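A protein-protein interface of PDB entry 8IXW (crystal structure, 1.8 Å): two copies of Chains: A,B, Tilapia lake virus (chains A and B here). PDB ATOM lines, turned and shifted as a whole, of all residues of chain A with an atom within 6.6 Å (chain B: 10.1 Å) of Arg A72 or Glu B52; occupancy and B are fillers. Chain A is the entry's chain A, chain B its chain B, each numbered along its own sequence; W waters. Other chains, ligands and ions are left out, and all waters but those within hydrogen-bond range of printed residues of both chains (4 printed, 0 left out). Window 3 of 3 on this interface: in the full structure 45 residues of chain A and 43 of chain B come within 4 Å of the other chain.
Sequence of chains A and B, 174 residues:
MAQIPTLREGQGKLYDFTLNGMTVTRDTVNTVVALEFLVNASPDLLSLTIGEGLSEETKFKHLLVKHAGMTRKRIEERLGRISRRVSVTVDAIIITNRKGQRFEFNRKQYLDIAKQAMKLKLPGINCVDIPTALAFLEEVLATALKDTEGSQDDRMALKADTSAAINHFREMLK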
ATOM      1  N   PRO A   5      -5.240  -5.868   3.788  1.00  0.00           N
ATOM      2  CA  PRO A   5      -5.673  -5.302   5.051  1.00  0.00           C
ATOM      3  C   PRO A   5      -7.144  -5.475   5.367  1.00  0.00           C
ATOM      4  O   PRO A   5      -7.518  -5.221   6.457  1.00  0.00           O
ATOM      5  CB  PRO A   5      -5.436  -3.791   4.965  1.00  0.00           C
ATOM      6  CG  PRO A   5      -5.234  -3.529   3.522  1.00  0.00           C
ATOM      7  CD  PRO A   5      -4.735  -4.818   2.926  1.00  0.00           C
ATOM      8  N   THR A   6      -7.924  -5.918   4.404  1.00  0.00           N
ATOM      9  CA  THR A   6      -9.360  -6.160   4.588  1.00  0.00           C
ATOM     10  C   THR A   6      -9.544  -7.613   5.043  1.00  0.00           C
ATOM     11  O   THR A   6     -10.275  -8.291   4.359  1.00  0.00           O
ATOM     12  CB  THR A   6     -10.095  -5.889   3.269  1.00  0.00           C
ATOM     13  OG1 THR A   6      -9.861  -7.058   2.492  1.00  0.00           O
ATOM     14  CG2 THR A   6      -9.602  -4.665   2.527  1.00  0.00           C
ATOM     15  N   LEU A   7      -8.982  -8.044   6.176  1.00  0.00           N
ATOM     16  CA  LEU A   7      -9.008  -9.453   6.662  1.00  0.00           C
ATOM     17  C   LEU A   7      -8.672 -10.350   5.467  1.00  0.00           C
ATOM     18  O   LEU A   7      -7.560 -10.873   5.429  1.00  0.00           O
ATOM     19  CB  LEU A   7     -10.381  -9.833   7.239  1.00  0.00           C
ATOM     20  CG  LEU A   7     -10.522  -9.875   8.756  1.00  0.00           C
ATOM     21  CD1 LEU A   7     -11.810  -9.189   9.172  1.00  0.00           C
ATOM     22  CD2 LEU A   7     -10.501 -11.305   9.262  1.00  0.00           C
ATOM     23  N   ASP A  16     -22.631 -13.982   6.152  1.00  0.00           N
ATOM     24  CA  ASP A  16     -23.510 -12.834   6.353  1.00  0.00           C
ATOM     25  C   ASP A  16     -23.799 -12.099   5.045  1.00  0.00           C
ATOM     26  O   ASP A  16     -23.998 -10.880   5.043  1.00  0.00           O
ATOM     27  CB  ASP A  16     -22.935 -11.871   7.393  1.00  0.00           C
ATOM     28  CG  ASP A  16     -21.468 -11.586   7.182  1.00  0.00           C
ATOM     29  OD1 ASP A  16     -20.934 -11.964   6.119  1.00  0.00           O
ATOM     30  OD2 ASP A  16     -20.846 -10.983   8.083  1.00  0.00           O
ATOM     31  N   PHE A  17     -23.850 -12.826   3.929  1.00  0.00           N
ATOM     32  CA  PHE A  17     -24.291 -12.279   2.653  1.00  0.00           C
ATOM     33  C   PHE A  17     -25.326 -13.212   2.040  1.00  0.00           C
ATOM     34  O   PHE A  17     -25.366 -14.406   2.340  1.00  0.00           O
ATOM     35  CB  PHE A  17     -23.121 -12.080   1.675  1.00  0.00           C
ATOM     36  CG  PHE A  17     -22.250 -10.897   2.001  1.00  0.00           C
ATOM     37  CD1 PHE A  17     -21.281 -10.984   2.987  1.00  0.00           C
ATOM     38  CD2 PHE A  17     -22.405  -9.699   1.324  1.00  0.00           C
ATOM     39  CE1 PHE A  17     -20.480  -9.897   3.290  1.00  0.00           C
ATOM     40  CE2 PHE A  17     -21.610  -8.610   1.623  1.00  0.00           C
ATOM     41  CZ  PHE A  17     -20.646  -8.708   2.608  1.00  0.00           C
ATOM     42  N   THR A  18     -26.168 -12.655   1.172  1.00  0.00           N
ATOM     43  CA  THR A  18     -27.227 -13.403   0.508  1.00  0.00           C
ATOM     44  C   THR A  18     -27.046 -13.328  -1.003  1.00  0.00           C
ATOM     45  O   THR A  18     -26.712 -12.270  -1.548  1.00  0.00           O
ATOM     46  CB  THR A  18     -28.621 -12.874   0.912  1.00  0.00           C
ATOM     47  OG1 THR A  18     -28.771 -12.950   2.336  1.00  0.00           O
ATOM     48  CG2 THR A  18     -29.741 -13.660   0.234  1.00  0.00           C
ATOM     49  N   ARG A  26     -18.414 -13.757   2.848  1.00  0.00           N
ATOM     50  CA  ARG A  26     -17.765 -12.711   2.065  1.00  0.00           C
ATOM     51  C   ARG A  26     -16.718 -13.309   1.133  1.00  0.00           C
ATOM     52  O   ARG A  26     -16.526 -12.825   0.013  1.00  0.00           O
ATOM     53  CB  ARG A  26     -17.133 -11.669   2.991  1.00  0.00           C
ATOM     54  CG  ARG A  26     -16.418 -10.529   2.262  1.00  0.00           C
ATOM     55  CD  ARG A  26     -17.381  -9.696   1.430  1.00  0.00           C
ATOM     56  NE  ARG A  26     -16.695  -8.775   0.530  1.00  0.00           N
ATOM     57  CZ  ARG A  26     -16.391  -7.516   0.813  1.00  0.00           C
ATOM     58  NH1 ARG A  26     -16.713  -6.967   1.973  1.00  0.00           N
ATOM     59  NH2 ARG A  26     -15.757  -6.783  -0.099  1.00  0.00           N
ATOM     60  N   MET A  70     -13.853  -3.845  -1.497  1.00  0.00           N
ATOM     61  CA  MET A  70     -15.115  -3.124  -1.597  1.00  0.00           C
ATOM     62  C   MET A  70     -15.849  -3.128  -0.258  1.00  0.00           C
ATOM     63  O   MET A  70     -15.715  -4.053   0.550  1.00  0.00           O
ATOM     64  CB  MET A  70     -15.997  -3.758  -2.677  1.00  0.00           C
ATOM     65  CG  MET A  70     -15.560  -3.486  -4.118  1.00  0.00           C
ATOM     66  SD  MET A  70     -16.389  -4.580  -5.294  1.00  0.00           S
ATOM     67  CE  MET A  70     -17.432  -3.447  -6.209  1.00  0.00           C
ATOM     68  N   THR A  71     -16.625  -2.074  -0.021  1.00  0.00           N
ATOM     69  CA  THR A  71     -17.492  -2.037   1.145  1.00  0.00           C
ATOM     70  C   THR A  71     -18.579  -3.102   1.022  1.00  0.00           C
ATOM     71  O   THR A  71     -18.916  -3.554  -0.075  1.00  0.00           O
ATOM     72  CB  THR A  71     -18.163  -0.672   1.290  1.00  0.00           C
ATOM     73  OG1 THR A  71     -18.903  -0.383   0.096  1.00  0.00           O
ATOM     74  CG2 THR A  71     -17.134   0.423   1.530  1.00  0.00           C
ATOM     75  N   ARG A  72     -19.146  -3.492   2.167  1.00  0.00           N
ATOM     76  CA  ARG A  72     -20.334  -4.342   2.129  1.00  0.00           C
ATOM     77  C   ARG A  72     -21.402  -3.718   1.241  1.00  0.00           C
ATOM     78  O   ARG A  72     -22.023  -4.396   0.415  1.00  0.00           O
ATOM     79  CB  ARG A  72     -20.891  -4.564   3.537  1.00  0.00           C
ATOM     80  CG  ARG A  72     -22.340  -5.061   3.535  1.00  0.00           C
ATOM     81  CD  ARG A  72     -22.897  -5.225   4.937  1.00  0.00           C
ATOM     82  NE  ARG A  72     -22.224  -6.299   5.654  1.00  0.00           N
ATOM     83  CZ  ARG A  72     -22.485  -7.588   5.490  1.00  0.00           C
ATOM     84  NH1 ARG A  72     -23.419  -8.004   4.650  1.00  0.00           N
ATOM     85  NH2 ARG A  72     -21.789  -8.483   6.186  1.00  0.00           N
ATOM     86  N   LYS A  73     -21.639  -2.415   1.418  1.00  0.00           N
ATOM     87  CA  LYS A  73     -22.683  -1.738   0.659  1.00  0.00           C
ATOM     88  C   LYS A  73     -22.443  -1.871  -0.836  1.00  0.00           C
ATOM     89  O   LYS A  73     -23.365  -2.174  -1.602  1.00  0.00           O
ATOM     90  CB  LYS A  73     -22.749  -0.265   1.071  1.00  0.00           C
ATOM     91  CG  LYS A  73     -23.502   0.634   0.100  1.00  0.00           C
ATOM     92  CD  LYS A  73     -23.489   2.086   0.570  1.00  0.00           C
ATOM     93  CE  LYS A  73     -24.364   2.960  -0.314  1.00  0.00           C
ATOM     94  NZ  LYS A  73     -23.766   4.308  -0.536  1.00  0.00           N
ATOM     95  N   ARG A  74     -21.205  -1.651  -1.274  1.00  0.00           N
ATOM     96  CA  ARG A  74     -20.935  -1.632  -2.706  1.00  0.00           C
ATOM     97  C   ARG A  74     -20.932  -3.038  -3.293  1.00  0.00           C
ATOM     98  O   ARG A  74     -21.387  -3.240  -4.425  1.00  0.00           O
ATOM     99  CB  ARG A  74     -19.605  -0.928  -2.970  1.00  0.00           C
ATOM    100  CG  ARG A  74     -19.222  -0.869  -4.427  1.00  0.00           C
ATOM    101  CD  ARG A  74     -18.687   0.502  -4.809  1.00  0.00           C
ATOM    102  NE  ARG A  74     -18.146   0.495  -6.161  1.00  0.00           N
ATOM    103  CZ  ARG A  74     -16.887   0.207  -6.460  1.00  0.00           C
ATOM    104  NH1 ARG A  74     -15.999  -0.077  -5.521  1.00  0.00           N
ATOM    105  NH2 ARG A  74     -16.508   0.203  -7.735  1.00  0.00           N
ATOM    106  N   ILE A  75     -20.448  -4.026  -2.541  1.00  0.00           N
ATOM    107  CA  ILE A  75     -20.452  -5.384  -3.073  1.00  0.00           C
ATOM    108  C   ILE A  75     -21.854  -5.989  -3.008  1.00  0.00           C
ATOM    109  O   ILE A  75     -22.190  -6.861  -3.815  1.00  0.00           O
ATOM    110  CB  ILE A  75     -19.411  -6.261  -2.351  1.00  0.00           C
ATOM    111  CG1 ILE A  75     -18.953  -7.384  -3.290  1.00  0.00           C
ATOM    112  CG2 ILE A  75     -19.973  -6.818  -1.061  1.00  0.00           C
ATOM    113  CD1 ILE A  75     -17.648  -8.036  -2.896  1.00  0.00           C
ATOM    114  N   GLU A  76     -22.700  -5.537  -2.078  1.00  0.00           N
ATOM    115  CA  GLU A  76     -24.102  -5.941  -2.122  1.00  0.00           C
ATOM    116  C   GLU A  76     -24.800  -5.347  -3.340  1.00  0.00           C
ATOM    117  O   GLU A  76     -25.648  -6.003  -3.960  1.00  0.00           O
ATOM    118  CB  GLU A  76     -24.818  -5.528  -0.835  1.00  0.00           C
ATOM    119  CG  GLU A  76     -24.521  -6.433   0.347  1.00  0.00           C
ATOM    120  CD  GLU A  76     -25.231  -6.002   1.616  1.00  0.00           C
ATOM    121  OE1 GLU A  76     -25.856  -4.920   1.611  1.00  0.00           O
ATOM    122  OE2 GLU A  76     -25.162  -6.745   2.617  1.00  0.00           O
ATOM    123  N   GLU A  77     -24.455  -4.108  -3.700  1.00  0.00           N
ATOM    124  CA  GLU A  77     -25.001  -3.512  -4.915  1.00  0.00           C
ATOM    125  C   GLU A  77     -24.557  -4.292  -6.144  1.00  0.00           C
ATOM    126  O   GLU A  77     -25.349  -4.522  -7.065  1.00  0.00           O
ATOM    127  CB  GLU A  77     -24.573  -2.051  -5.026  1.00  0.00           C
ATOM    128  CG  GLU A  77     -24.464  -1.524  -6.452  1.00  0.00           C
ATOM    129  CD  GLU A  77     -24.428  -0.004  -6.511  1.00  0.00           C
ATOM    130  OE1 GLU A  77     -24.430   0.635  -5.435  1.00  0.00           O
ATOM    131  OE2 GLU A  77     -24.396   0.553  -7.628  1.00  0.00           O
ATOM    132  N   SER B  42     -13.122   8.460   1.910  1.00  0.00           N
ATOM    133  CA  SER B  42     -14.382   7.883   1.475  1.00  0.00           C
ATOM    134  C   SER B  42     -14.567   6.521   2.144  1.00  0.00           C
ATOM    135  O   SER B  42     -13.589   5.856   2.505  1.00  0.00           O
ATOM    136  CB  SER B  42     -14.421   7.746  -0.044  1.00  0.00           C
ATOM    137  OG  SER B  42     -13.454   6.825  -0.505  1.00  0.00           O
ATOM    138  N   PRO B  43     -15.810   6.091   2.352  1.00  0.00           N
ATOM    139  CA  PRO B  43     -16.023   4.726   2.863  1.00  0.00           C
ATOM    140  C   PRO B  43     -15.320   3.676   2.021  1.00  0.00           C
ATOM    141  O   PRO B  43     -14.843   2.671   2.564  1.00  0.00           O
ATOM    142  CB  PRO B  43     -17.549   4.578   2.829  1.00  0.00           C
ATOM    143  CG  PRO B  43     -18.058   5.982   2.945  1.00  0.00           C
ATOM    144  CD  PRO B  43     -17.079   6.819   2.168  1.00  0.00           C
ATOM    145  N   ASP B  44     -15.222   3.895   0.707  1.00  0.00           N
ATOM    146  CA  ASP B  44     -14.501   2.961  -0.150  1.00  0.00           C
ATOM    147  C   ASP B  44     -13.020   2.918   0.218  1.00  0.00           C
ATOM    148  O   ASP B  44     -12.428   1.841   0.337  1.00  0.00           O
ATOM    149  CB  ASP B  44     -14.678   3.354  -1.620  1.00  0.00           C
ATOM    150  CG  ASP B  44     -16.137   3.402  -2.047  1.00  0.00           C
ATOM    151  OD1 ASP B  44     -16.891   2.453  -1.749  1.00  0.00           O
ATOM    152  OD2 ASP B  44     -16.532   4.396  -2.689  1.00  0.00           O
ATOM    153  N   LEU B  45     -12.406   4.089   0.411  1.00  0.00           N
ATOM    154  CA  LEU B  45     -10.998   4.124   0.798  1.00  0.00           C
ATOM    155  C   LEU B  45     -10.788   3.515   2.181  1.00  0.00           C
ATOM    156  O   LEU B  45      -9.827   2.770   2.397  1.00  0.00           O
ATOM    157  CB  LEU B  45     -10.474   5.561   0.764  1.00  0.00           C
ATOM    158  CG  LEU B  45      -8.953   5.719   0.885  1.00  0.00           C
ATOM    159  CD1 LEU B  45      -8.220   4.948  -0.208  1.00  0.00           C
ATOM    160  CD2 LEU B  45      -8.556   7.196   0.862  1.00  0.00           C
ATOM    161  N   LEU B  46     -11.667   3.830   3.137  1.00  0.00           N
ATOM    162  CA  LEU B  46     -11.530   3.257   4.472  1.00  0.00           C
ATOM    163  C   LEU B  46     -11.575   1.734   4.427  1.00  0.00           C
ATOM    164  O   LEU B  46     -10.784   1.059   5.097  1.00  0.00           O
ATOM    165  CB  LEU B  46     -12.626   3.793   5.392  1.00  0.00           C
ATOM    166  CG  LEU B  46     -12.338   3.744   6.893  1.00  0.00           C
ATOM    167  CD1 LEU B  46     -11.127   4.599   7.248  1.00  0.00           C
ATOM    168  CD2 LEU B  46     -13.557   4.186   7.699  1.00  0.00           C
ATOM    169  N   SER B  47     -12.498   1.174   3.645  1.00  0.00           N
ATOM    170  CA  SER B  47     -12.594  -0.279   3.542  1.00  0.00           C
ATOM    171  C   SER B  47     -11.309  -0.875   2.985  1.00  0.00           C
ATOM    172  O   SER B  47     -10.831  -1.908   3.468  1.00  0.00           O
ATOM    173  CB  SER B  47     -13.783  -0.660   2.661  1.00  0.00           C
ATOM    174  OG  SER B  47     -14.105  -2.029   2.811  1.00  0.00           O
ATOM    175  N   LEU B  48     -10.742  -0.239   1.961  1.00  0.00           N
ATOM    176  CA  LEU B  48      -9.494  -0.721   1.383  1.00  0.00           C
ATOM    177  C   LEU B  48      -8.358  -0.677   2.399  1.00  0.00           C
ATOM    178  O   LEU B  48      -7.496  -1.563   2.417  1.00  0.00           O
ATOM    179  CB  LEU B  48      -9.143   0.112   0.151  1.00  0.00           C
ATOM    180  CG  LEU B  48      -9.926  -0.172  -1.129  1.00  0.00           C
ATOM    181  CD1 LEU B  48      -9.725   0.929  -2.157  1.00  0.00           C
ATOM    182  CD2 LEU B  48      -9.500  -1.511  -1.717  1.00  0.00           C
ATOM    183  N   THR B  49      -8.347   0.334   3.269  1.00  0.00           N
ATOM    184  CA  THR B  49      -7.175   0.590   4.093  1.00  0.00           C
ATOM    185  C   THR B  49      -7.211  -0.118   5.443  1.00  0.00           C
ATOM    186  O   THR B  49      -6.158  -0.554   5.924  1.00  0.00           O
ATOM    187  CB  THR B  49      -6.998   2.103   4.297  1.00  0.00           C
ATOM    188  OG1 THR B  49      -8.109   2.628   5.030  1.00  0.00           O
ATOM    189  CG2 THR B  49      -6.898   2.812   2.954  1.00  0.00           C
ATOM    190  N   ILE B  50      -8.381  -0.258   6.074  1.00  0.00           N
ATOM    191  CA  ILE B  50      -8.430  -0.897   7.387  1.00  0.00           C
ATOM    192  C   ILE B  50      -9.451  -2.024   7.458  1.00  0.00           C
ATOM    193  O   ILE B  50      -9.533  -2.731   8.471  1.00  0.00           O
ATOM    194  CB  ILE B  50      -8.728   0.134   8.502  1.00  0.00           C
ATOM    195  CG1 ILE B  50     -10.075   0.823   8.265  1.00  0.00           C
ATOM    196  CG2 ILE B  50      -7.609   1.151   8.600  1.00  0.00           C
ATOM    197  CD1 ILE B  50     -10.584   1.594   9.474  1.00  0.00           C
ATOM    198  N   GLY B  51     -10.236  -2.195   6.405  1.00  0.00           N
ATOM    199  CA  GLY B  51     -11.300  -3.179   6.419  1.00  0.00           C
ATOM    200  C   GLY B  51     -12.556  -2.635   7.077  1.00  0.00           C
ATOM    201  O   GLY B  51     -12.645  -1.471   7.461  1.00  0.00           O
ATOM    202  N   GLU B  52     -13.550  -3.506   7.195  1.00  0.00           N
ATOM    203  CA  GLU B  52     -14.811  -3.196   7.858  1.00  0.00           C
ATOM    204  C   GLU B  52     -14.961  -4.109   9.071  1.00  0.00           C
ATOM    205  O   GLU B  52     -14.075  -4.899   9.386  1.00  0.00           O
ATOM    206  CB  GLU B  52     -15.987  -3.348   6.896  1.00  0.00           C
ATOM    207  CG  GLU B  52     -16.237  -2.112   6.051  1.00  0.00           C
ATOM    208  CD  GLU B  52     -17.455  -2.250   5.167  1.00  0.00           C
ATOM    209  OE1 GLU B  52     -17.693  -3.363   4.655  1.00  0.00           O
ATOM    210  OE2 GLU B  52     -18.176  -1.243   4.983  1.00  0.00           O
ATOM    211  N   GLY B  53     -16.091  -4.001   9.758  1.00  0.00           N
ATOM    212  CA  GLY B  53     -16.311  -4.799  10.938  1.00  0.00           C
ATOM    213  C   GLY B  53     -15.582  -4.322  12.170  1.00  0.00           C
ATOM    214  O   GLY B  53     -15.487  -5.071  13.150  1.00  0.00           O
ATOM    215  N   LEU B  54     -15.062  -3.102  12.159  1.00  0.00           N
ATOM    216  CA  LEU B  54     -14.361  -2.541  13.300  1.00  0.00           C
ATOM    217  C   LEU B  54     -15.232  -1.502  13.992  1.00  0.00           C
ATOM    218  O   LEU B  54     -15.954  -0.742  13.336  1.00  0.00           O
ATOM    219  CB  LEU B  54     -13.036  -1.903  12.878  1.00  0.00           C
ATOM    220  CG  LEU B  54     -12.041  -2.834  12.186  1.00  0.00           C
ATOM    221  CD1 LEU B  54     -10.786  -2.070  11.783  1.00  0.00           C
ATOM    222  CD2 LEU B  54     -11.707  -4.006  13.095  1.00  0.00           C
ATOM    223  N   SER B  55     -15.167  -1.482  15.319  1.00  0.00           N
ATOM    224  CA  SER B  55     -15.820  -0.435  16.082  1.00  0.00           C
ATOM    225  C   SER B  55     -15.164   0.909  15.785  1.00  0.00           C
ATOM    226  O   SER B  55     -14.057   0.986  15.247  1.00  0.00           O
ATOM    227  CB  SER B  55     -15.742  -0.731  17.574  1.00  0.00           C
ATOM    228  OG  SER B  55     -14.392  -0.745  18.004  1.00  0.00           O
ATOM    229  N   GLU B  56     -15.858   1.983  16.159  1.00  0.00           N
ATOM    230  CA  GLU B  56     -15.346   3.321  15.878  1.00  0.00           C
ATOM    231  C   GLU B  56     -13.993   3.546  16.541  1.00  0.00           C
ATOM    232  O   GLU B  56     -13.083   4.118  15.929  1.00  0.00           O
ATOM    233  CB  GLU B  56     -16.357   4.371  16.334  1.00  0.00           C
ATOM    234  CG  GLU B  56     -17.614   4.405  15.478  1.00  0.00           C
ATOM    235  CD  GLU B  56     -17.311   4.673  14.015  1.00  0.00           C
ATOM    236  OE1 GLU B  56     -16.693   5.718  13.721  1.00  0.00           O
ATOM    237  OE2 GLU B  56     -17.680   3.835  13.165  1.00  0.00           O
ATOM    238  N   THR B  58     -11.816   1.220  17.316  1.00  0.00           N
ATOM    239  CA  THR B  58     -10.822   0.357  16.687  1.00  0.00           C
ATOM    240  C   THR B  58     -10.418   0.887  15.316  1.00  0.00           C
ATOM    241  O   THR B  58      -9.253   0.765  14.919  1.00  0.00           O
ATOM    242  CB  THR B  58     -11.366  -1.068  16.583  1.00  0.00           C
ATOM    243  OG1 THR B  58     -11.778  -1.516  17.881  1.00  0.00           O
ATOM    244  CG2 THR B  58     -10.303  -2.007  16.054  1.00  0.00           C
ATOM    245  N   LYS B  59     -11.359   1.479  14.579  1.00  0.00           N
ATOM    246  CA  LYS B  59     -11.005   2.137  13.327  1.00  0.00           C
ATOM    247  C   LYS B  59      -9.910   3.173  13.555  1.00  0.00           C
ATOM    248  O   LYS B  59      -8.926   3.235  12.812  1.00  0.00           O
ATOM    249  CB  LYS B  59     -12.234   2.797  12.703  1.00  0.00           C
ATOM    250  CG  LYS B  59     -13.171   1.850  11.967  1.00  0.00           C
ATOM    251  CD  LYS B  59     -14.200   2.644  11.177  1.00  0.00           C
ATOM    252  CE  LYS B  59     -15.621   2.245  11.530  1.00  0.00           C
ATOM    253  NZ  LYS B  59     -16.568   2.587  10.431  1.00  0.00           N
ATOM    254  N   HIS B  62      -6.468   1.435  14.460  1.00  0.00           N
ATOM    255  CA  HIS B  62      -5.791   0.923  13.270  1.00  0.00           C
ATOM    256  C   HIS B  62      -5.230   2.055  12.420  1.00  0.00           C
ATOM    257  O   HIS B  62      -4.095   1.972  11.938  1.00  0.00           O
ATOM    258  CB  HIS B  62      -6.776   0.071  12.461  1.00  0.00           C
ATOM    259  CG  HIS B  62      -6.969  -1.307  13.012  1.00  0.00           C
ATOM    260  ND1 HIS B  62      -7.715  -1.555  14.144  1.00  0.00           N
ATOM    261  CD2 HIS B  62      -6.560  -2.516  12.559  1.00  0.00           C
ATOM    262  CE1 HIS B  62      -7.713  -2.851  14.392  1.00  0.00           C
ATOM    263  NE2 HIS B  62      -7.030  -3.457  13.438  1.00  0.00           N
HETATM  264  O   HOH W   1     -19.465   2.137  -0.694  1.00  0.00           O
HETATM  265  O   HOH W   2     -20.518  -0.805   3.918  1.00  0.00           O
HETATM  266  O   HOH W   3     -15.844  -4.938   3.842  1.00  0.00           O
HETATM  267  O   HOH W   4     -16.061   0.041  -2.009  1.00  0.00           O
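The side-chain hydroxyl of Ser B47 lies within hydrogen-bond range of the backbone carbonyl oxygen of Met A70, at 3.4 Å. The side-chain carboxylate (OE1) of Glu B52 sits at hydrogen-bond distance from the backbone NH (N) of Arg A72 (2.9 Å).
NH1 of Arg A72 lies within salt-bridge range of OE2 of Glu A76. O of Leu B46 is in hydrogen-bond range of OG1 of Thr B49 (3.1 Å). The backbone carbonyl oxygen (O) of Leu B45 sits close to the side-chain hydroxyl (OG1) of Thr B49, 3.1 Å away. OG1 of Thr A71 lies within hydrogen-bond range of N of Arg A74 (3.0 Å). The guanidinium group (NH2) of Arg A26 is in hydrogen-bond range of the backbone carbonyl oxygen (O) of Met A70, 2.8 Å away. The side-chain carboxylate of Asp A16 is in salt-bridge range of the guanidinium group of Arg A72, at 3.3 Å.
Pro A5 touches Leu B48. Thr B49 touches Pro A5 (O to CB, 3.5 Å). Pro A5 touches Ile B50 (O to O, 3.8 Å). Thr A6 touches Ser B47. O of Leu B48 touches CG2 of Thr A6 (3.8 Å). Thr A71 touches Pro B43 (CG2 to O, 3.4 Å). Thr A71 touches Asp B44. Ser B47 touches Thr A71. CB of Thr A71 touches OE2 of Glu B52, 3.7 Å away.
No residue of chain B comes within 4 Å of Asp A16. Arg A72 touches just one residue of chain B: Glu B52 (2.9 Å). Ser B42 touches none of the printed residues of chain A. Of the printed residues of chain A, Pro B43 touches Thr A71. Printed residues of chain A within 4 Å of Thr B49: Pro A5 (3.5 Å). Of chain A, only Thr A71 and Arg A72 come within 4 Å of Glu B52. The nearest residue of chain B that does not touch Arg A72 is Ser B47 (5.3 Å). The nearest printed residue of chain A that does not touch Pro B43 is Met A70 (6.5 Å).
Hydrophobic or aromatic side chains of chain A that line the printed part of chain B: Pro A5. Of the 18 printed residues of chain B, 7 touch a printed residue of chain A.
No position is printed for both chains. Of the 11 pairs that touch across the chains among the printed residues, none has its exchanged pair printed and touching as well.
Water W3 lies within hydrogen-bond range of the side-chain carboxylate (OE1) of Glu B52 (2.6 Å), the guanidinium group (NH1) of Arg A26 (2.9 Å) and the backbone carbonyl oxygen (O) of Met A70 (3.4 Å). Water W4 bridges the side-chain carboxylate (OD1) of Asp B44 (2.6 Å) and the backbone NH (N) of Thr A71 (3.0 Å). Water W2 lies within hydrogen-bond range of OE2 of Glu B52 (2.6 Å), N of Lys A73 (3.2 Å) and N of Arg A72 (3.5 Å). Water W1 bridges OG1 of Thr A71 and OD1 of Asp B44.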
